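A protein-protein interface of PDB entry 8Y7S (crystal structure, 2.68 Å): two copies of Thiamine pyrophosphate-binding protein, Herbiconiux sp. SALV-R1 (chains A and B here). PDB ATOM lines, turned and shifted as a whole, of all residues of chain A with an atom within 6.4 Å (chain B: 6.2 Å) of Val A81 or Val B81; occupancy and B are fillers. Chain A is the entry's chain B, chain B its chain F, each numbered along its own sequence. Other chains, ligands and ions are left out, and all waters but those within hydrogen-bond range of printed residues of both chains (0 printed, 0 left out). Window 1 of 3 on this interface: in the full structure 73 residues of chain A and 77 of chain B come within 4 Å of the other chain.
OG1 of Thr A78 is in hydrogen-bond range of OG1 of Thr B82, 2.9 Å away.
The side-chain sulfur of Met B50 sits close to the side-chain amide oxygen of Asn A79 (3.6 Å).
The side-chain amide oxygen of Asn A79 sits at hydrogen-bond distance from the side-chain hydroxyl of Thr B82 (2.7 Å).
The side-chain hydroxyl (OG1) of Thr A82 is in hydrogen-bond range of the side-chain hydroxyl (OG1) of Thr B78, 2.6 Å away.
OD1 of Asn B79 sits at hydrogen-bond distance from OG1 of Thr A82 (2.7 Å).
The backbone carbonyl oxygen (O) of Asn A79 sits close to the backbone NH (N) of Met A50 (3.4 Å).
N of Met B50 lies close to O of Asn B79, at 3.5 Å.
OD1 of Asn B79 touches SD of Met A50, at 3.8 Å.
CB of Ala B85 touches CG2 of Thr A78, at 3.99 Å.
CG1 of Val A81 touches CG2 of Val B81 (3.9 Å).
Ala A85 touches Thr B78.
CG2 of Ile A120 touches CG2 of Ile B120 (3.6 Å).
Ile A124 touches Ile B120 (CG2 to CD1, 3.8 Å).
Of the printed residues of chain B, Val A81 touches Val B81 (3.9 Å).
Val B81 touches just one residue of chain A: Val A81 (3.9 Å).
Of the printed residues of chain B, Ile A124 touches Ile B120 (3.8 Å).
Of the printed residues of chain A, Thr B82 touches Thr A78 (2.9 Å) and Asn A79 (2.7 Å).
Printed residues of chain A within 4 Å of Ala B85: Thr A78 (3.99 Å).
Printed residues of chain B within 4 Å of Ile A120: Ile B120 (3.6 Å).
Printed residues of chain B within 4 Å of Asn A79: Met B50 and Thr B82.
Ser B83 touches none of the printed residues of chain A.
The nearest printed residue of chain B that does not touch Val A81 is Thr B78 (4.01 Å).
The nearest residue of chain A that does not touch Val B81 is Thr A78 (4.3 Å).
Hydrophobic or aromatic side chains of chain A that line the printed part of chain B: Met A50, Val A81, Ala A85, Ile A120 and Ile A124.
Of the 13 printed residues of chain B, 7 touch a printed residue of chain A.
Printed residues of chain B that touch a printed residue of chain A: Met B50, Thr B78, Asn B79, Val B81, Thr B82, Ala B85 and Ile B120.
Among the printed residues, 11 pairs touch across the chains.
Among the printed residues, no Asp or Glu carboxylate lies within 4 Å of a Lys or Arg side-chain nitrogen of the other chain.
Thr A78 touches Thr B82, and with the chains exchanged Thr A82 touches Thr B78.
Asn A79 touches Thr B82, and with the chains exchanged Thr A82 touches Asn B79.
Val B81 touches its own counterpart, Val A81.
Ile A124 touches Ile B120, but with the chains exchanged Ile A120 does not touch Ile B124 (4.1 Å).
Positions printed for both chains: 50, 77, 78, 79, 80, 81, 82, 83, 84, 85, 86, 120 and 124.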
ATOM      1  N   MET A  50       5.336 -17.361 -21.095  1.00  0.00           N
ATOM      2  CA  MET A  50       5.160 -18.617 -20.375  1.00  0.00           C
ATOM      3  C   MET A  50       4.623 -19.704 -21.293  1.00  0.00           C
ATOM      4  O   MET A  50       5.090 -20.849 -21.250  1.00  0.00           O
ATOM      5  CB  MET A  50       4.273 -18.414 -19.139  1.00  0.00           C
ATOM      6  CG  MET A  50       2.805 -18.770 -19.237  1.00  0.00           C
ATOM      7  SD  MET A  50       2.080 -19.131 -17.619  1.00  0.00           S
ATOM      8  CE  MET A  50       0.382 -19.397 -18.103  1.00  0.00           C
ATOM      9  N   PHE A  77      12.350 -13.299 -20.559  1.00  0.00           N
ATOM     10  CA  PHE A  77      12.936 -14.475 -19.925  1.00  0.00           C
ATOM     11  C   PHE A  77      12.151 -14.895 -18.688  1.00  0.00           C
ATOM     12  O   PHE A  77      11.808 -16.072 -18.534  1.00  0.00           O
ATOM     13  CB  PHE A  77      14.395 -14.212 -19.554  1.00  0.00           C
ATOM     14  CG  PHE A  77      14.917 -15.152 -18.511  1.00  0.00           C
ATOM     15  CD1 PHE A  77      15.349 -16.416 -18.867  1.00  0.00           C
ATOM     16  CD2 PHE A  77      14.957 -14.783 -17.179  1.00  0.00           C
ATOM     17  CE1 PHE A  77      15.812 -17.291 -17.923  1.00  0.00           C
ATOM     18  CE2 PHE A  77      15.416 -15.656 -16.228  1.00  0.00           C
ATOM     19  CZ  PHE A  77      15.846 -16.917 -16.602  1.00  0.00           C
ATOM     20  N   THR A  78      11.879 -13.951 -17.781  1.00  0.00           N
ATOM     21  CA  THR A  78      11.302 -14.319 -16.486  1.00  0.00           C
ATOM     22  C   THR A  78       9.928 -14.966 -16.623  1.00  0.00           C
ATOM     23  O   THR A  78       9.582 -15.841 -15.819  1.00  0.00           O
ATOM     24  CB  THR A  78      11.212 -13.103 -15.560  1.00  0.00           C
ATOM     25  OG1 THR A  78      10.378 -12.099 -16.151  1.00  0.00           O
ATOM     26  CG2 THR A  78      12.593 -12.522 -15.277  1.00  0.00           C
ATOM     27  N   ASN A  79       9.126 -14.547 -17.612  1.00  0.00           N
ATOM     28  CA  ASN A  79       7.812 -15.154 -17.822  1.00  0.00           C
ATOM     29  C   ASN A  79       7.907 -16.626 -18.215  1.00  0.00           C
ATOM     30  O   ASN A  79       6.914 -17.347 -18.093  1.00  0.00           O
ATOM     31  CB  ASN A  79       7.008 -14.374 -18.868  1.00  0.00           C
ATOM     32  CG  ASN A  79       6.320 -13.141 -18.283  1.00  0.00           C
ATOM     33  OD1 ASN A  79       5.850 -13.161 -17.139  1.00  0.00           O
ATOM     34  ND2 ASN A  79       6.241 -12.065 -19.069  1.00  0.00           N
ATOM     35  N   ALA A  80       9.061 -17.081 -18.690  1.00  0.00           N
ATOM     36  CA  ALA A  80       9.234 -18.467 -19.114  1.00  0.00           C
ATOM     37  C   ALA A  80       9.714 -19.399 -18.001  1.00  0.00           C
ATOM     38  O   ALA A  80       9.860 -20.603 -18.245  1.00  0.00           O
ATOM     39  CB  ALA A  80      10.219 -18.532 -20.282  1.00  0.00           C
ATOM     40  N   VAL A  81       9.937 -18.885 -16.788  1.00  0.00           N
ATOM     41  CA  VAL A  81      10.613 -19.675 -15.759  1.00  0.00           C
ATOM     42  C   VAL A  81       9.806 -20.914 -15.385  1.00  0.00           C
ATOM     43  O   VAL A  81      10.374 -21.986 -15.143  1.00  0.00           O
ATOM     44  CB  VAL A  81      10.908 -18.791 -14.534  1.00  0.00           C
ATOM     45  CG1 VAL A  81      11.253 -19.651 -13.318  1.00  0.00           C
ATOM     46  CG2 VAL A  81      12.033 -17.819 -14.864  1.00  0.00           C
ATOM     47  N   THR A  82       8.474 -20.793 -15.318  1.00  0.00           N
ATOM     48  CA  THR A  82       7.648 -21.956 -14.996  1.00  0.00           C
ATOM     49  C   THR A  82       7.825 -23.066 -16.027  1.00  0.00           C
ATOM     50  O   THR A  82       7.907 -24.247 -15.669  1.00  0.00           O
ATOM     51  CB  THR A  82       6.171 -21.557 -14.879  1.00  0.00           C
ATOM     52  OG1 THR A  82       5.989 -20.687 -13.755  1.00  0.00           O
ATOM     53  CG2 THR A  82       5.283 -22.789 -14.691  1.00  0.00           C
ATOM     54  N   SER A  83       7.907 -22.708 -17.311  1.00  0.00           N
ATOM     55  CA  SER A  83       8.092 -23.727 -18.339  1.00  0.00           C
ATOM     56  C   SER A  83       9.442 -24.414 -18.186  1.00  0.00           C
ATOM     57  O   SER A  83       9.534 -25.646 -18.273  1.00  0.00           O
ATOM     58  CB  SER A  83       7.947 -23.099 -19.729  1.00  0.00           C
ATOM     59  OG  SER A  83       8.593 -23.874 -20.723  1.00  0.00           O
ATOM     60  N   ILE A  84      10.495 -23.634 -17.927  1.00  0.00           N
ATOM     61  CA  ILE A  84      11.809 -24.211 -17.664  1.00  0.00           C
ATOM     62  C   ILE A  84      11.728 -25.173 -16.486  1.00  0.00           C
ATOM     63  O   ILE A  84      12.213 -26.308 -16.557  1.00  0.00           O
ATOM     64  CB  ILE A  84      12.841 -23.097 -17.419  1.00  0.00           C
ATOM     65  CG1 ILE A  84      12.885 -22.133 -18.610  1.00  0.00           C
ATOM     66  CG2 ILE A  84      14.203 -23.684 -17.171  1.00  0.00           C
ATOM     67  CD1 ILE A  84      13.773 -20.928 -18.385  1.00  0.00           C
ATOM     68  N   ALA A  85      11.091 -24.739 -15.393  1.00  0.00           N
ATOM     69  CA  ALA A  85      10.939 -25.605 -14.226  1.00  0.00           C
ATOM     70  C   ALA A  85      10.137 -26.852 -14.563  1.00  0.00           C
ATOM     71  O   ALA A  85      10.473 -27.958 -14.122  1.00  0.00           O
ATOM     72  CB  ALA A  85      10.266 -24.840 -13.089  1.00  0.00           C
ATOM     73  N   ASN A  86       9.075 -26.695 -15.347  1.00  0.00           N
ATOM     74  CA  ASN A  86       8.259 -27.838 -15.731  1.00  0.00           C
ATOM     75  C   ASN A  86       9.054 -28.810 -16.595  1.00  0.00           C
ATOM     76  O   ASN A  86       9.002 -30.028 -16.386  1.00  0.00           O
ATOM     77  CB  ASN A  86       7.004 -27.352 -16.454  1.00  0.00           C
ATOM     78  CG  ASN A  86       5.940 -28.421 -16.552  1.00  0.00           C
ATOM     79  OD1 ASN A  86       5.603 -29.083 -15.565  1.00  0.00           O
ATOM     80  ND2 ASN A  86       5.427 -28.621 -17.755  1.00  0.00           N
ATOM     81  N   ILE A 120      19.194 -17.295 -12.401  1.00  0.00           N
ATOM     82  CA  ILE A 120      17.811 -17.692 -12.142  1.00  0.00           C
ATOM     83  C   ILE A 120      17.541 -19.065 -12.730  1.00  0.00           C
ATOM     84  O   ILE A 120      16.870 -19.898 -12.123  1.00  0.00           O
ATOM     85  CB  ILE A 120      16.825 -16.651 -12.702  1.00  0.00           C
ATOM     86  CG1 ILE A 120      16.956 -15.333 -11.956  1.00  0.00           C
ATOM     87  CG2 ILE A 120      15.388 -17.153 -12.623  1.00  0.00           C
ATOM     88  CD1 ILE A 120      16.435 -14.181 -12.735  1.00  0.00           C
ATOM     89  N   ALA A 121      18.066 -19.320 -13.917  1.00  0.00           N
ATOM     90  CA  ALA A 121      17.778 -20.557 -14.622  1.00  0.00           C
ATOM     91  C   ALA A 121      18.616 -21.727 -14.131  1.00  0.00           C
ATOM     92  O   ALA A 121      18.190 -22.876 -14.299  1.00  0.00           O
ATOM     93  CB  ALA A 121      17.989 -20.363 -16.125  1.00  0.00           C
ATOM     94  N   ILE A 124      17.240 -24.952 -12.414  1.00  0.00           N
ATOM     95  CA  ILE A 124      16.226 -25.708 -13.132  1.00  0.00           C
ATOM     96  C   ILE A 124      16.645 -26.006 -14.573  1.00  0.00           C
ATOM     97  O   ILE A 124      15.795 -26.223 -15.431  1.00  0.00           O
ATOM     98  CB  ILE A 124      14.864 -24.991 -13.082  1.00  0.00           C
ATOM     99  CG1 ILE A 124      15.015 -23.536 -13.541  1.00  0.00           C
ATOM    100  CG2 ILE A 124      14.285 -25.072 -11.666  1.00  0.00           C
ATOM    101  CD1 ILE A 124      13.794 -22.682 -13.305  1.00  0.00           C
ATOM    102  N   LEU A 416       6.115 -31.122 -11.285  1.00  0.00           N
ATOM    103  CA  LEU A 416       5.821 -29.741 -10.919  1.00  0.00           C
ATOM    104  C   LEU A 416       4.332 -29.538 -10.678  1.00  0.00           C
ATOM    105  O   LEU A 416       3.940 -28.746  -9.814  1.00  0.00           O
ATOM    106  CB  LEU A 416       6.322 -28.787 -12.000  1.00  0.00           C
ATOM    107  CG  LEU A 416       6.175 -27.321 -11.594  1.00  0.00           C
ATOM    108  CD1 LEU A 416       7.078 -27.046 -10.411  1.00  0.00           C
ATOM    109  CD2 LEU A 416       6.508 -26.399 -12.748  1.00  0.00           C
ATOM    110  N   MET B  50       1.369 -14.874 -11.338  1.00  0.00           N
ATOM    111  CA  MET B  50       2.082 -13.709 -11.848  1.00  0.00           C
ATOM    112  C   MET B  50       1.379 -12.416 -11.440  1.00  0.00           C
ATOM    113  O   MET B  50       2.027 -11.457 -11.000  1.00  0.00           O
ATOM    114  CB  MET B  50       2.212 -13.817 -13.368  1.00  0.00           C
ATOM    115  CG  MET B  50       2.225 -12.501 -14.120  1.00  0.00           C
ATOM    116  SD  MET B  50       2.506 -12.750 -15.888  1.00  0.00           S
ATOM    117  CE  MET B  50       1.007 -12.082 -16.586  1.00  0.00           C
ATOM    118  N   PHE B  77       5.206 -20.677  -7.139  1.00  0.00           N
ATOM    119  CA  PHE B  77       6.327 -19.756  -6.964  1.00  0.00           C
ATOM    120  C   PHE B  77       6.869 -19.293  -8.311  1.00  0.00           C
ATOM    121  O   PHE B  77       7.082 -18.090  -8.526  1.00  0.00           O
ATOM    122  CB  PHE B  77       7.442 -20.392  -6.138  1.00  0.00           C
ATOM    123  CG  PHE B  77       8.785 -19.762  -6.373  1.00  0.00           C
ATOM    124  CD1 PHE B  77       9.077 -18.521  -5.828  1.00  0.00           C
ATOM    125  CD2 PHE B  77       9.736 -20.381  -7.170  1.00  0.00           C
ATOM    126  CE1 PHE B  77      10.294 -17.912  -6.057  1.00  0.00           C
ATOM    127  CE2 PHE B  77      10.963 -19.776  -7.410  1.00  0.00           C
ATOM    128  CZ  PHE B  77      11.242 -18.539  -6.850  1.00  0.00           C
ATOM    129  N   THR B  78       7.130 -20.232  -9.226  1.00  0.00           N
ATOM    130  CA  THR B  78       7.804 -19.864 -10.471  1.00  0.00           C
ATOM    131  C   THR B  78       6.981 -18.873 -11.289  1.00  0.00           C
ATOM    132  O   THR B  78       7.549 -18.001 -11.954  1.00  0.00           O
ATOM    133  CB  THR B  78       8.110 -21.114 -11.307  1.00  0.00           C
ATOM    134  OG1 THR B  78       6.893 -21.798 -11.637  1.00  0.00           O
ATOM    135  CG2 THR B  78       9.029 -22.055 -10.547  1.00  0.00           C
ATOM    136  N   ASN B  79       5.649 -18.972 -11.241  1.00  0.00           N
ATOM    137  CA  ASN B  79       4.820 -18.037 -11.990  1.00  0.00           C
ATOM    138  C   ASN B  79       4.977 -16.600 -11.507  1.00  0.00           C
ATOM    139  O   ASN B  79       4.616 -15.671 -12.238  1.00  0.00           O
ATOM    140  CB  ASN B  79       3.350 -18.468 -11.932  1.00  0.00           C
ATOM    141  CG  ASN B  79       3.004 -19.503 -12.991  1.00  0.00           C
ATOM    142  OD1 ASN B  79       3.551 -19.479 -14.094  1.00  0.00           O
ATOM    143  ND2 ASN B  79       2.090 -20.407 -12.675  1.00  0.00           N
ATOM    144  N   ALA B  80       5.466 -16.394 -10.288  1.00  0.00           N
ATOM    145  CA  ALA B  80       5.634 -15.058  -9.728  1.00  0.00           C
ATOM    146  C   ALA B  80       7.021 -14.458  -9.971  1.00  0.00           C
ATOM    147  O   ALA B  80       7.282 -13.343  -9.505  1.00  0.00           O
ATOM    148  CB  ALA B  80       5.330 -15.071  -8.230  1.00  0.00           C
ATOM    149  N   VAL B  81       7.922 -15.170 -10.656  1.00  0.00           N
ATOM    150  CA  VAL B  81       9.309 -14.712 -10.769  1.00  0.00           C
ATOM    151  C   VAL B  81       9.379 -13.372 -11.499  1.00  0.00           C
ATOM    152  O   VAL B  81      10.194 -12.503 -11.161  1.00  0.00           O
ATOM    153  CB  VAL B  81      10.169 -15.782 -11.459  1.00  0.00           C
ATOM    154  CG1 VAL B  81      11.527 -15.221 -11.815  1.00  0.00           C
ATOM    155  CG2 VAL B  81      10.298 -17.008 -10.563  1.00  0.00           C
ATOM    156  N   THR B  82       8.530 -13.190 -12.516  1.00  0.00           N
ATOM    157  CA  THR B  82       8.478 -11.924 -13.243  1.00  0.00           C
ATOM    158  C   THR B  82       8.143 -10.765 -12.312  1.00  0.00           C
ATOM    159  O   THR B  82       8.724  -9.678 -12.424  1.00  0.00           O
ATOM    160  CB  THR B  82       7.435 -12.015 -14.361  1.00  0.00           C
ATOM    161  OG1 THR B  82       7.813 -13.028 -15.298  1.00  0.00           O
ATOM    162  CG2 THR B  82       7.295 -10.689 -15.084  1.00  0.00           C
ATOM    163  N   SER B  83       7.207 -10.982 -11.386  1.00  0.00           N
ATOM    164  CA  SER B  83       6.845  -9.938 -10.434  1.00  0.00           C
ATOM    165  C   SER B  83       8.004  -9.613  -9.502  1.00  0.00           C
ATOM    166  O   SER B  83       8.279  -8.436  -9.234  1.00  0.00           O
ATOM    167  CB  SER B  83       5.618 -10.374  -9.631  1.00  0.00           C
ATOM    168  OG  SER B  83       5.432  -9.551  -8.495  1.00  0.00           O
ATOM    169  N   ILE B  84       8.693 -10.643  -8.998  1.00  0.00           N
ATOM    170  CA  ILE B  84       9.852 -10.419  -8.140  1.00  0.00           C
ATOM    171  C   ILE B  84      10.902  -9.596  -8.871  1.00  0.00           C
ATOM    172  O   ILE B  84      11.415  -8.599  -8.345  1.00  0.00           O
ATOM    173  CB  ILE B  84      10.433 -11.758  -7.655  1.00  0.00           C
ATOM    174  CG1 ILE B  84       9.357 -12.623  -7.005  1.00  0.00           C
ATOM    175  CG2 ILE B  84      11.563 -11.508  -6.695  1.00  0.00           C
ATOM    176  CD1 ILE B  84       9.745 -14.077  -6.865  1.00  0.00           C
ATOM    177  N   ALA B  85      11.230  -9.998 -10.101  1.00  0.00           N
ATOM    178  CA  ALA B  85      12.228  -9.270 -10.875  1.00  0.00           C
ATOM    179  C   ALA B  85      11.796  -7.829 -11.117  1.00  0.00           C
ATOM    180  O   ALA B  85      12.621  -6.909 -11.074  1.00  0.00           O
ATOM    181  CB  ALA B  85      12.495  -9.985 -12.198  1.00  0.00           C
ATOM    182  N   ASN B  86      10.507  -7.612 -11.377  1.00  0.00           N
ATOM    183  CA  ASN B  86      10.024  -6.257 -11.608  1.00  0.00           C
ATOM    184  C   ASN B  86      10.186  -5.407 -10.353  1.00  0.00           C
ATOM    185  O   ASN B  86      10.724  -4.294 -10.406  1.00  0.00           O
ATOM    186  CB  ASN B  86       8.565  -6.307 -12.063  1.00  0.00           C
ATOM    187  CG  ASN B  86       8.097  -5.000 -12.657  1.00  0.00           C
ATOM    188  OD1 ASN B  86       8.696  -4.471 -13.596  1.00  0.00           O
ATOM    189  ND2 ASN B  86       7.025  -4.457 -12.097  1.00  0.00           N
ATOM    190  N   ILE B 120      16.559 -19.651  -7.094  1.00  0.00           N
ATOM    191  CA  ILE B 120      15.942 -18.976  -8.232  1.00  0.00           C
ATOM    192  C   ILE B 120      15.640 -17.520  -7.898  1.00  0.00           C
ATOM    193  O   ILE B 120      15.775 -16.635  -8.751  1.00  0.00           O
ATOM    194  CB  ILE B 120      14.686 -19.741  -8.679  1.00  0.00           C
ATOM    195  CG1 ILE B 120      15.074 -21.170  -9.051  1.00  0.00           C
ATOM    196  CG2 ILE B 120      14.003 -19.035  -9.843  1.00  0.00           C
ATOM    197  CD1 ILE B 120      13.940 -22.005  -9.512  1.00  0.00           C
ATOM    198  N   ILE B 124      17.206 -11.804  -7.725  1.00  0.00           N
ATOM    199  CA  ILE B 124      16.246 -10.719  -7.911  1.00  0.00           C
ATOM    200  C   ILE B 124      15.551 -10.347  -6.607  1.00  0.00           C
ATOM    201  O   ILE B 124      14.415  -9.860  -6.619  1.00  0.00           O
ATOM    202  CB  ILE B 124      15.216 -11.063  -9.001  1.00  0.00           C
ATOM    203  CG1 ILE B 124      14.783 -12.523  -8.903  1.00  0.00           C
ATOM    204  CG2 ILE B 124      15.792 -10.783 -10.369  1.00  0.00           C
ATOM    205  CD1 ILE B 124      13.765 -12.915  -9.955  1.00  0.00           C
